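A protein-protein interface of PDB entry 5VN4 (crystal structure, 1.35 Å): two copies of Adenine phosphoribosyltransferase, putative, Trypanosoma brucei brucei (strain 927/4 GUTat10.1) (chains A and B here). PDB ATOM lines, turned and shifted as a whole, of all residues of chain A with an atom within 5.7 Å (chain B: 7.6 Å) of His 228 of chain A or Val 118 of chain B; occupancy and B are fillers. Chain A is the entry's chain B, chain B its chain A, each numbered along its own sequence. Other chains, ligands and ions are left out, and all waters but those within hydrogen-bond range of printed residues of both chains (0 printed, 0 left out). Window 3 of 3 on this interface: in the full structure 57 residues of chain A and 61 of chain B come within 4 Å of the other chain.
Printed residues of chain B within 4 Å of Pro 225 of chain A: Val 118 (3.8 Å). Printed residues of chain B within 4 Å of His 228 of chain A: Val 118. Lys 229 of chain A touches none of the printed residues of chain B. Printed residues of chain B within 4 Å of Arg 232 of chain A: Ile 115, Ala 116, Gly 117, Val 118 and Ile 119. Printed residues of chain A within 4 Å of Ile 115 of chain B: Arg 232 (2.8 Å). Printed residues of chain A within 4 Å of Ala 116 of chain B: Phe 42 and Arg 232. Printed residues of chain A within 4 Å of Val 118 of chain B: Pro 225 (3.8 Å), His 228 (3.7 Å) and Arg 232 (3.2 Å). Of the printed residues of chain A, Ile 120 of chain B touches Ile 234. The nearest printed residue of chain B that does not touch Phe 42 of chain A is Ile 115 of chain B (5.0 Å).
Of the 11 printed residues of chain B, 6 touch a printed residue of chain A. Hydrophobic or aromatic side chains of chain B that line the printed part of chain A: Ala 116, Val 118, Ile 119 and Ile 120. Hydrophobic or aromatic side chains of chain A that line the printed part of chain B: Pro 225, His 228, Ile 233 and Ile 234. Among the printed residues, 12 pairs touch across the chains.
No position is printed for both chains.
The backbone NH of Phe 141 of chain B is in hydrogen-bond range of the backbone carbonyl oxygen of Val 118 of chain B, 2.8 Å away. The backbone carbonyl oxygen (O) of Val 139 of chain B is in hydrogen-bond range of the backbone NH (N) of Ile 120 of chain B, at 2.9 Å. O of Ser 231 of chain A sits at hydrogen-bond distance from NE2 of His 228 of chain A, at 2.8 Å. OG of Ser 231 of chain A lies within hydrogen-bond range of N of Ile 233 of chain A, at 3.1 Å.
Among the printed residues, pairs that only touch across the chains: Arg 232 of chain A with Val 118 of chain B, Phe 42 of chain A with Ala 116 of chain B, Ile 234 of chain A with Ile 120 of chain B, Ile 233 of chain A with Ile 119 of chain B, His 228 of chain A with Val 118 of chain B, Arg 232 of chain A with Ala 116 of chain B and Pro 225 of chain A with Val 118 of chain B.
The backbone carbonyl oxygen (O) of Ile 115 of chain B lies within hydrogen-bond range of the guanidinium group (NH1) of Arg 232 of chain A (2.8 Å). The backbone carbonyl oxygen (O) of Phe 42 of chain A lies within hydrogen-bond range of the backbone NH (N) of Gly 117 of chain B (2.7 Å). The guanidinium group (NH1) of Arg 232 of chain A sits at hydrogen-bond distance from the backbone carbonyl oxygen (O) of Gly 117 of chain B, at 2.9 Å. The backbone NH (N) of Ile 119 of chain B lies within hydrogen-bond range of the backbone carbonyl oxygen (O) of Arg 232 of chain A (2.9 Å). N of Ile 234 of chain A is in hydrogen-bond range of O of Ile 119 of chain B (2.8 Å).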
ATOM      1  N   PHE A  42     -16.814  -3.280 -12.449  1.00  0.00           N
ATOM      2  CA  PHE A  42     -17.633  -2.224 -13.032  1.00  0.00           C
ATOM      3  C   PHE A  42     -17.028  -1.665 -14.313  1.00  0.00           C
ATOM      4  O   PHE A  42     -17.389  -0.562 -14.737  1.00  0.00           O
ATOM      5  CB  PHE A  42     -17.892  -1.110 -12.017  1.00  0.00           C
ATOM      6  CG  PHE A  42     -18.756  -1.535 -10.866  1.00  0.00           C
ATOM      7  CD1 PHE A  42     -20.127  -1.656 -11.024  1.00  0.00           C
ATOM      8  CD2 PHE A  42     -18.203  -1.824  -9.628  1.00  0.00           C
ATOM      9  CE1 PHE A  42     -20.925  -2.056  -9.973  1.00  0.00           C
ATOM     10  CE2 PHE A  42     -19.001  -2.223  -8.572  1.00  0.00           C
ATOM     11  CZ  PHE A  42     -20.363  -2.337  -8.746  1.00  0.00           C
ATOM     12  N   PRO A 225     -20.189   2.095  -8.192  1.00  0.00           N
ATOM     13  CA  PRO A 225     -21.440   2.276  -7.442  1.00  0.00           C
ATOM     14  C   PRO A 225     -21.538   1.265  -6.309  1.00  0.00           C
ATOM     15  O   PRO A 225     -21.834   0.086  -6.522  1.00  0.00           O
ATOM     16  CB  PRO A 225     -22.517   2.050  -8.513  1.00  0.00           C
ATOM     17  CG  PRO A 225     -21.879   1.155  -9.493  1.00  0.00           C
ATOM     18  CD  PRO A 225     -20.424   1.533  -9.535  1.00  0.00           C
ATOM     19  N   LEU A 226     -21.315   1.738  -5.086  1.00  0.00           N
ATOM     20  CA  LEU A 226     -21.129   0.864  -3.935  1.00  0.00           C
ATOM     21  C   LEU A 226     -22.410   0.169  -3.485  1.00  0.00           C
ATOM     22  O   LEU A 226     -22.331  -0.775  -2.693  1.00  0.00           O
ATOM     23  CB  LEU A 226     -20.543   1.681  -2.779  1.00  0.00           C
ATOM     24  CG  LEU A 226     -19.033   1.665  -2.513  1.00  0.00           C
ATOM     25  CD1 LEU A 226     -18.240   1.384  -3.742  1.00  0.00           C
ATOM     26  CD2 LEU A 226     -18.579   2.967  -1.873  1.00  0.00           C
ATOM     27  N   HIS A 227     -23.578   0.607  -3.954  1.00  0.00           N
ATOM     28  CA  HIS A 227     -24.847   0.025  -3.537  1.00  0.00           C
ATOM     29  C   HIS A 227     -25.564  -0.722  -4.650  1.00  0.00           C
ATOM     30  O   HIS A 227     -26.582  -1.368  -4.378  1.00  0.00           O
ATOM     31  CB  HIS A 227     -25.784   1.115  -2.995  1.00  0.00           C
ATOM     32  CG  HIS A 227     -25.384   1.661  -1.658  1.00  0.00           C
ATOM     33  ND1 HIS A 227     -25.866   1.155  -0.468  1.00  0.00           N
ATOM     34  CD2 HIS A 227     -24.571   2.693  -1.326  1.00  0.00           C
ATOM     35  CE1 HIS A 227     -25.360   1.846   0.539  1.00  0.00           C
ATOM     36  NE2 HIS A 227     -24.566   2.781   0.045  1.00  0.00           N
ATOM     37  N   HIS A 228     -25.076  -0.652  -5.885  1.00  0.00           N
ATOM     38  CA  HIS A 228     -25.806  -1.219  -7.008  1.00  0.00           C
ATOM     39  C   HIS A 228     -25.871  -2.738  -6.901  1.00  0.00           C
ATOM     40  O   HIS A 228     -24.854  -3.401  -6.696  1.00  0.00           O
ATOM     41  CB  HIS A 228     -25.134  -0.830  -8.320  1.00  0.00           C
ATOM     42  CG  HIS A 228     -25.835  -1.377  -9.520  1.00  0.00           C
ATOM     43  ND1 HIS A 228     -27.039  -0.874  -9.967  1.00  0.00           N
ATOM     44  CD2 HIS A 228     -25.529  -2.410 -10.339  1.00  0.00           C
ATOM     45  CE1 HIS A 228     -27.432  -1.562 -11.025  1.00  0.00           C
ATOM     46  NE2 HIS A 228     -26.531  -2.495 -11.274  1.00  0.00           N
ATOM     47  N   LYS A 229     -27.070  -3.289  -7.045  1.00  0.00           N
ATOM     48  CA  LYS A 229     -27.290  -4.721  -6.917  1.00  0.00           C
ATOM     49  C   LYS A 229     -27.468  -5.347  -8.295  1.00  0.00           C
ATOM     50  O   LYS A 229     -28.150  -4.789  -9.158  1.00  0.00           O
ATOM     51  CB  LYS A 229     -28.536  -4.990  -6.069  1.00  0.00           C
ATOM     52  CG  LYS A 229     -28.498  -4.360  -4.678  1.00  0.00           C
ATOM     53  CD  LYS A 229     -27.422  -4.993  -3.814  1.00  0.00           C
ATOM     54  CE  LYS A 229     -27.499  -4.519  -2.372  1.00  0.00           C
ATOM     55  NZ  LYS A 229     -27.322  -3.057  -2.256  1.00  0.00           N
ATOM     56  N   GLY A 230     -26.852  -6.511  -8.494  1.00  0.00           N
ATOM     57  CA  GLY A 230     -27.018  -7.248  -9.730  1.00  0.00           C
ATOM     58  C   GLY A 230     -26.105  -6.749 -10.839  1.00  0.00           C
ATOM     59  O   GLY A 230     -25.118  -6.042 -10.613  1.00  0.00           O
ATOM     60  N   SER A 231     -26.457  -7.132 -12.065  1.00  0.00           N
ATOM     61  CA  SER A 231     -25.660  -6.764 -13.229  1.00  0.00           C
ATOM     62  C   SER A 231     -25.583  -5.250 -13.380  1.00  0.00           C
ATOM     63  O   SER A 231     -26.569  -4.536 -13.173  1.00  0.00           O
ATOM     64  CB  SER A 231     -26.275  -7.366 -14.492  1.00  0.00           C
ATOM     65  OG  SER A 231     -25.544  -6.966 -15.641  1.00  0.00           O
ATOM     66  N   ARG A 232     -24.399  -4.761 -13.758  1.00  0.00           N
ATOM     67  CA  ARG A 232     -24.233  -3.344 -14.055  1.00  0.00           C
ATOM     68  C   ARG A 232     -24.859  -2.939 -15.383  1.00  0.00           C
ATOM     69  O   ARG A 232     -24.971  -1.738 -15.649  1.00  0.00           O
ATOM     70  CB  ARG A 232     -22.752  -2.954 -14.038  1.00  0.00           C
ATOM     71  CG  ARG A 232     -21.971  -3.402 -15.271  1.00  0.00           C
ATOM     72  CD  ARG A 232     -20.488  -3.073 -15.126  1.00  0.00           C
ATOM     73  NE  ARG A 232     -19.724  -3.448 -16.312  1.00  0.00           N
ATOM     74  CZ  ARG A 232     -19.507  -2.639 -17.342  1.00  0.00           C
ATOM     75  NH1 ARG A 232     -19.999  -1.406 -17.331  1.00  0.00           N
ATOM     76  NH2 ARG A 232     -18.794  -3.058 -18.381  1.00  0.00           N
ATOM     77  N   ILE A 233     -25.270  -3.896 -16.212  1.00  0.00           N
ATOM     78  CA  ILE A 233     -25.929  -3.614 -17.483  1.00  0.00           C
ATOM     79  C   ILE A 233     -27.427  -3.799 -17.277  1.00  0.00           C
ATOM     80  O   ILE A 233     -27.879  -4.887 -16.899  1.00  0.00           O
ATOM     81  CB  ILE A 233     -25.412  -4.544 -18.593  1.00  0.00           C
ATOM     82  CG1 ILE A 233     -23.886  -4.444 -18.705  1.00  0.00           C
ATOM     83  CG2 ILE A 233     -26.084  -4.222 -19.932  1.00  0.00           C
ATOM     84  CD1 ILE A 233     -23.263  -5.501 -19.597  1.00  0.00           C
ATOM     85  N   ILE A 234     -28.202  -2.743 -17.515  1.00  0.00           N
ATOM     86  CA  ILE A 234     -29.646  -2.794 -17.323  1.00  0.00           C
ATOM     87  C   ILE A 234     -30.353  -2.535 -18.648  1.00  0.00           C
ATOM     88  O   ILE A 234     -29.841  -1.833 -19.526  1.00  0.00           O
ATOM     89  CB  ILE A 234     -30.132  -1.834 -16.209  1.00  0.00           C
ATOM     90  CG1 ILE A 234     -29.947  -0.371 -16.618  1.00  0.00           C
ATOM     91  CG2 ILE A 234     -29.376  -2.101 -14.908  1.00  0.00           C
ATOM     92  CD1 ILE A 234     -30.503   0.615 -15.609  1.00  0.00           C
ATOM     93  N   ILE B 115     -18.264   1.005 -21.924  1.00  0.00           N
ATOM     94  CA  ILE B 115     -18.481   2.033 -20.911  1.00  0.00           C
ATOM     95  C   ILE B 115     -18.455   1.378 -19.540  1.00  0.00           C
ATOM     96  O   ILE B 115     -19.037   0.303 -19.347  1.00  0.00           O
ATOM     97  CB  ILE B 115     -19.840   2.724 -21.129  1.00  0.00           C
ATOM     98  CG1 ILE B 115     -19.943   3.293 -22.540  1.00  0.00           C
ATOM     99  CG2 ILE B 115     -20.078   3.799 -20.066  1.00  0.00           C
ATOM    100  CD1 ILE B 115     -21.302   3.898 -22.830  1.00  0.00           C
ATOM    101  N   ALA B 116     -17.814   2.040 -18.579  1.00  0.00           N
ATOM    102  CA  ALA B 116     -17.739   1.561 -17.207  1.00  0.00           C
ATOM    103  C   ALA B 116     -18.918   2.064 -16.374  1.00  0.00           C
ATOM    104  O   ALA B 116     -19.607   3.020 -16.739  1.00  0.00           O
ATOM    105  CB  ALA B 116     -16.431   2.025 -16.572  1.00  0.00           C
ATOM    106  N   GLY B 117     -19.129   1.416 -15.227  1.00  0.00           N
ATOM    107  CA  GLY B 117     -20.230   1.770 -14.342  1.00  0.00           C
ATOM    108  C   GLY B 117     -21.530   1.075 -14.713  1.00  0.00           C
ATOM    109  O   GLY B 117     -21.558   0.064 -15.424  1.00  0.00           O
ATOM    110  N   VAL B 118     -22.630   1.631 -14.214  1.00  0.00           N
ATOM    111  CA  VAL B 118     -23.957   1.133 -14.563  1.00  0.00           C
ATOM    112  C   VAL B 118     -24.347   1.718 -15.910  1.00  0.00           C
ATOM    113  O   VAL B 118     -24.249   2.931 -16.122  1.00  0.00           O
ATOM    114  CB  VAL B 118     -24.978   1.498 -13.474  1.00  0.00           C
ATOM    115  CG1 VAL B 118     -26.381   1.063 -13.887  1.00  0.00           C
ATOM    116  CG2 VAL B 118     -24.590   0.853 -12.142  1.00  0.00           C
ATOM    117  N   ILE B 119     -24.764   0.857 -16.836  1.00  0.00           N
ATOM    118  CA  ILE B 119     -25.050   1.287 -18.198  1.00  0.00           C
ATOM    119  C   ILE B 119     -26.380   0.706 -18.652  1.00  0.00           C
ATOM    120  O   ILE B 119     -26.807  -0.355 -18.188  1.00  0.00           O
ATOM    121  CB  ILE B 119     -23.912   0.943 -19.190  1.00  0.00           C
ATOM    122  CG1 ILE B 119     -23.790  -0.571 -19.384  1.00  0.00           C
ATOM    123  CG2 ILE B 119     -22.593   1.521 -18.710  1.00  0.00           C
ATOM    124  CD1 ILE B 119     -22.674  -0.975 -20.353  1.00  0.00           C
ATOM    125  N   ILE B 120     -27.040   1.425 -19.562  1.00  0.00           N
ATOM    126  CA  ILE B 120     -28.305   1.007 -20.159  1.00  0.00           C
ATOM    127  C   ILE B 120     -28.005   0.474 -21.551  1.00  0.00           C
ATOM    128  O   ILE B 120     -27.272   1.111 -22.312  1.00  0.00           O
ATOM    129  CB  ILE B 120     -29.279   2.193 -20.259  1.00  0.00           C
ATOM    130  CG1 ILE B 120     -29.415   2.924 -18.923  1.00  0.00           C
ATOM    131  CG2 ILE B 120     -30.633   1.729 -20.793  1.00  0.00           C
ATOM    132  CD1 ILE B 120     -30.126   4.243 -19.067  1.00  0.00           C
ATOM    133  N   VAL B 139     -25.315   3.358 -22.973  1.00  0.00           N
ATOM    134  CA  VAL B 139     -25.035   4.699 -22.464  1.00  0.00           C
ATOM    135  C   VAL B 139     -24.923   4.611 -20.949  1.00  0.00           C
ATOM    136  O   VAL B 139     -25.563   3.769 -20.309  1.00  0.00           O
ATOM    137  CB  VAL B 139     -26.113   5.714 -22.924  1.00  0.00           C
ATOM    138  CG1 VAL B 139     -27.433   5.504 -22.179  1.00  0.00           C
ATOM    139  CG2 VAL B 139     -25.607   7.139 -22.801  1.00  0.00           C
ATOM    140  N   ARG B 140     -24.089   5.470 -20.366  1.00  0.00           N
ATOM    141  CA  ARG B 140     -23.891   5.468 -18.922  1.00  0.00           C
ATOM    142  C   ARG B 140     -25.171   5.916 -18.227  1.00  0.00           C
ATOM    143  O   ARG B 140     -25.745   6.946 -18.588  1.00  0.00           O
ATOM    144  CB  ARG B 140     -22.759   6.440 -18.576  1.00  0.00           C
ATOM    145  CG  ARG B 140     -22.088   6.213 -17.236  1.00  0.00           C
ATOM    146  CD  ARG B 140     -20.919   7.181 -17.039  1.00  0.00           C
ATOM    147  NE  ARG B 140     -21.366   8.573 -17.003  1.00  0.00           N
ATOM    148  CZ  ARG B 140     -21.917   9.151 -15.939  1.00  0.00           C
ATOM    149  NH1 ARG B 140     -22.089   8.461 -14.817  1.00  0.00           N
ATOM    150  NH2 ARG B 140     -22.301  10.419 -15.991  1.00  0.00           N
ATOM    151  N   PHE B 141     -25.614   5.153 -17.233  1.00  0.00           N
ATOM    152  CA  PHE B 141     -26.734   5.593 -16.419  1.00  0.00           C
ATOM    153  C   PHE B 141     -26.319   6.814 -15.608  1.00  0.00           C
ATOM    154  O   PHE B 141     -25.229   6.846 -15.026  1.00  0.00           O
ATOM    155  CB  PHE B 141     -27.186   4.481 -15.478  1.00  0.00           C
ATOM    156  CG  PHE B 141     -28.408   4.836 -14.688  1.00  0.00           C
ATOM    157  CD1 PHE B 141     -29.666   4.718 -15.253  1.00  0.00           C
ATOM    158  CD2 PHE B 141     -28.302   5.315 -13.390  1.00  0.00           C
ATOM    159  CE1 PHE B 141     -30.797   5.053 -14.537  1.00  0.00           C
ATOM    160  CE2 PHE B 141     -29.434   5.651 -12.669  1.00  0.00           C
ATOM    161  CZ  PHE B 141     -30.682   5.521 -13.248  1.00  0.00           C
ATOM    162  N   GLY B 142     -27.172   7.829 -15.598  1.00  0.00           N
ATOM    163  CA  GLY B 142     -26.896   9.052 -14.881  1.00  0.00           C
ATOM    164  C   GLY B 142     -26.225  10.136 -15.693  1.00  0.00           C
ATOM    165  O   GLY B 142     -25.975  11.225 -15.155  1.00  0.00           O
ATOM    166  N   SER B 143     -25.918   9.881 -16.965  1.00  0.00           N
ATOM    167  CA  SER B 143     -25.319  10.907 -17.810  1.00  0.00           C
ATOM    168  C   SER B 143     -26.328  11.944 -18.279  1.00  0.00           C
ATOM    169  O   SER B 143     -25.932  13.057 -18.638  1.00  0.00           O
ATOM    170  CB  SER B 143     -24.597  10.266 -18.997  1.00  0.00           C
ATOM    171  OG  SER B 143     -25.454   9.387 -19.707  1.00  0.00           O
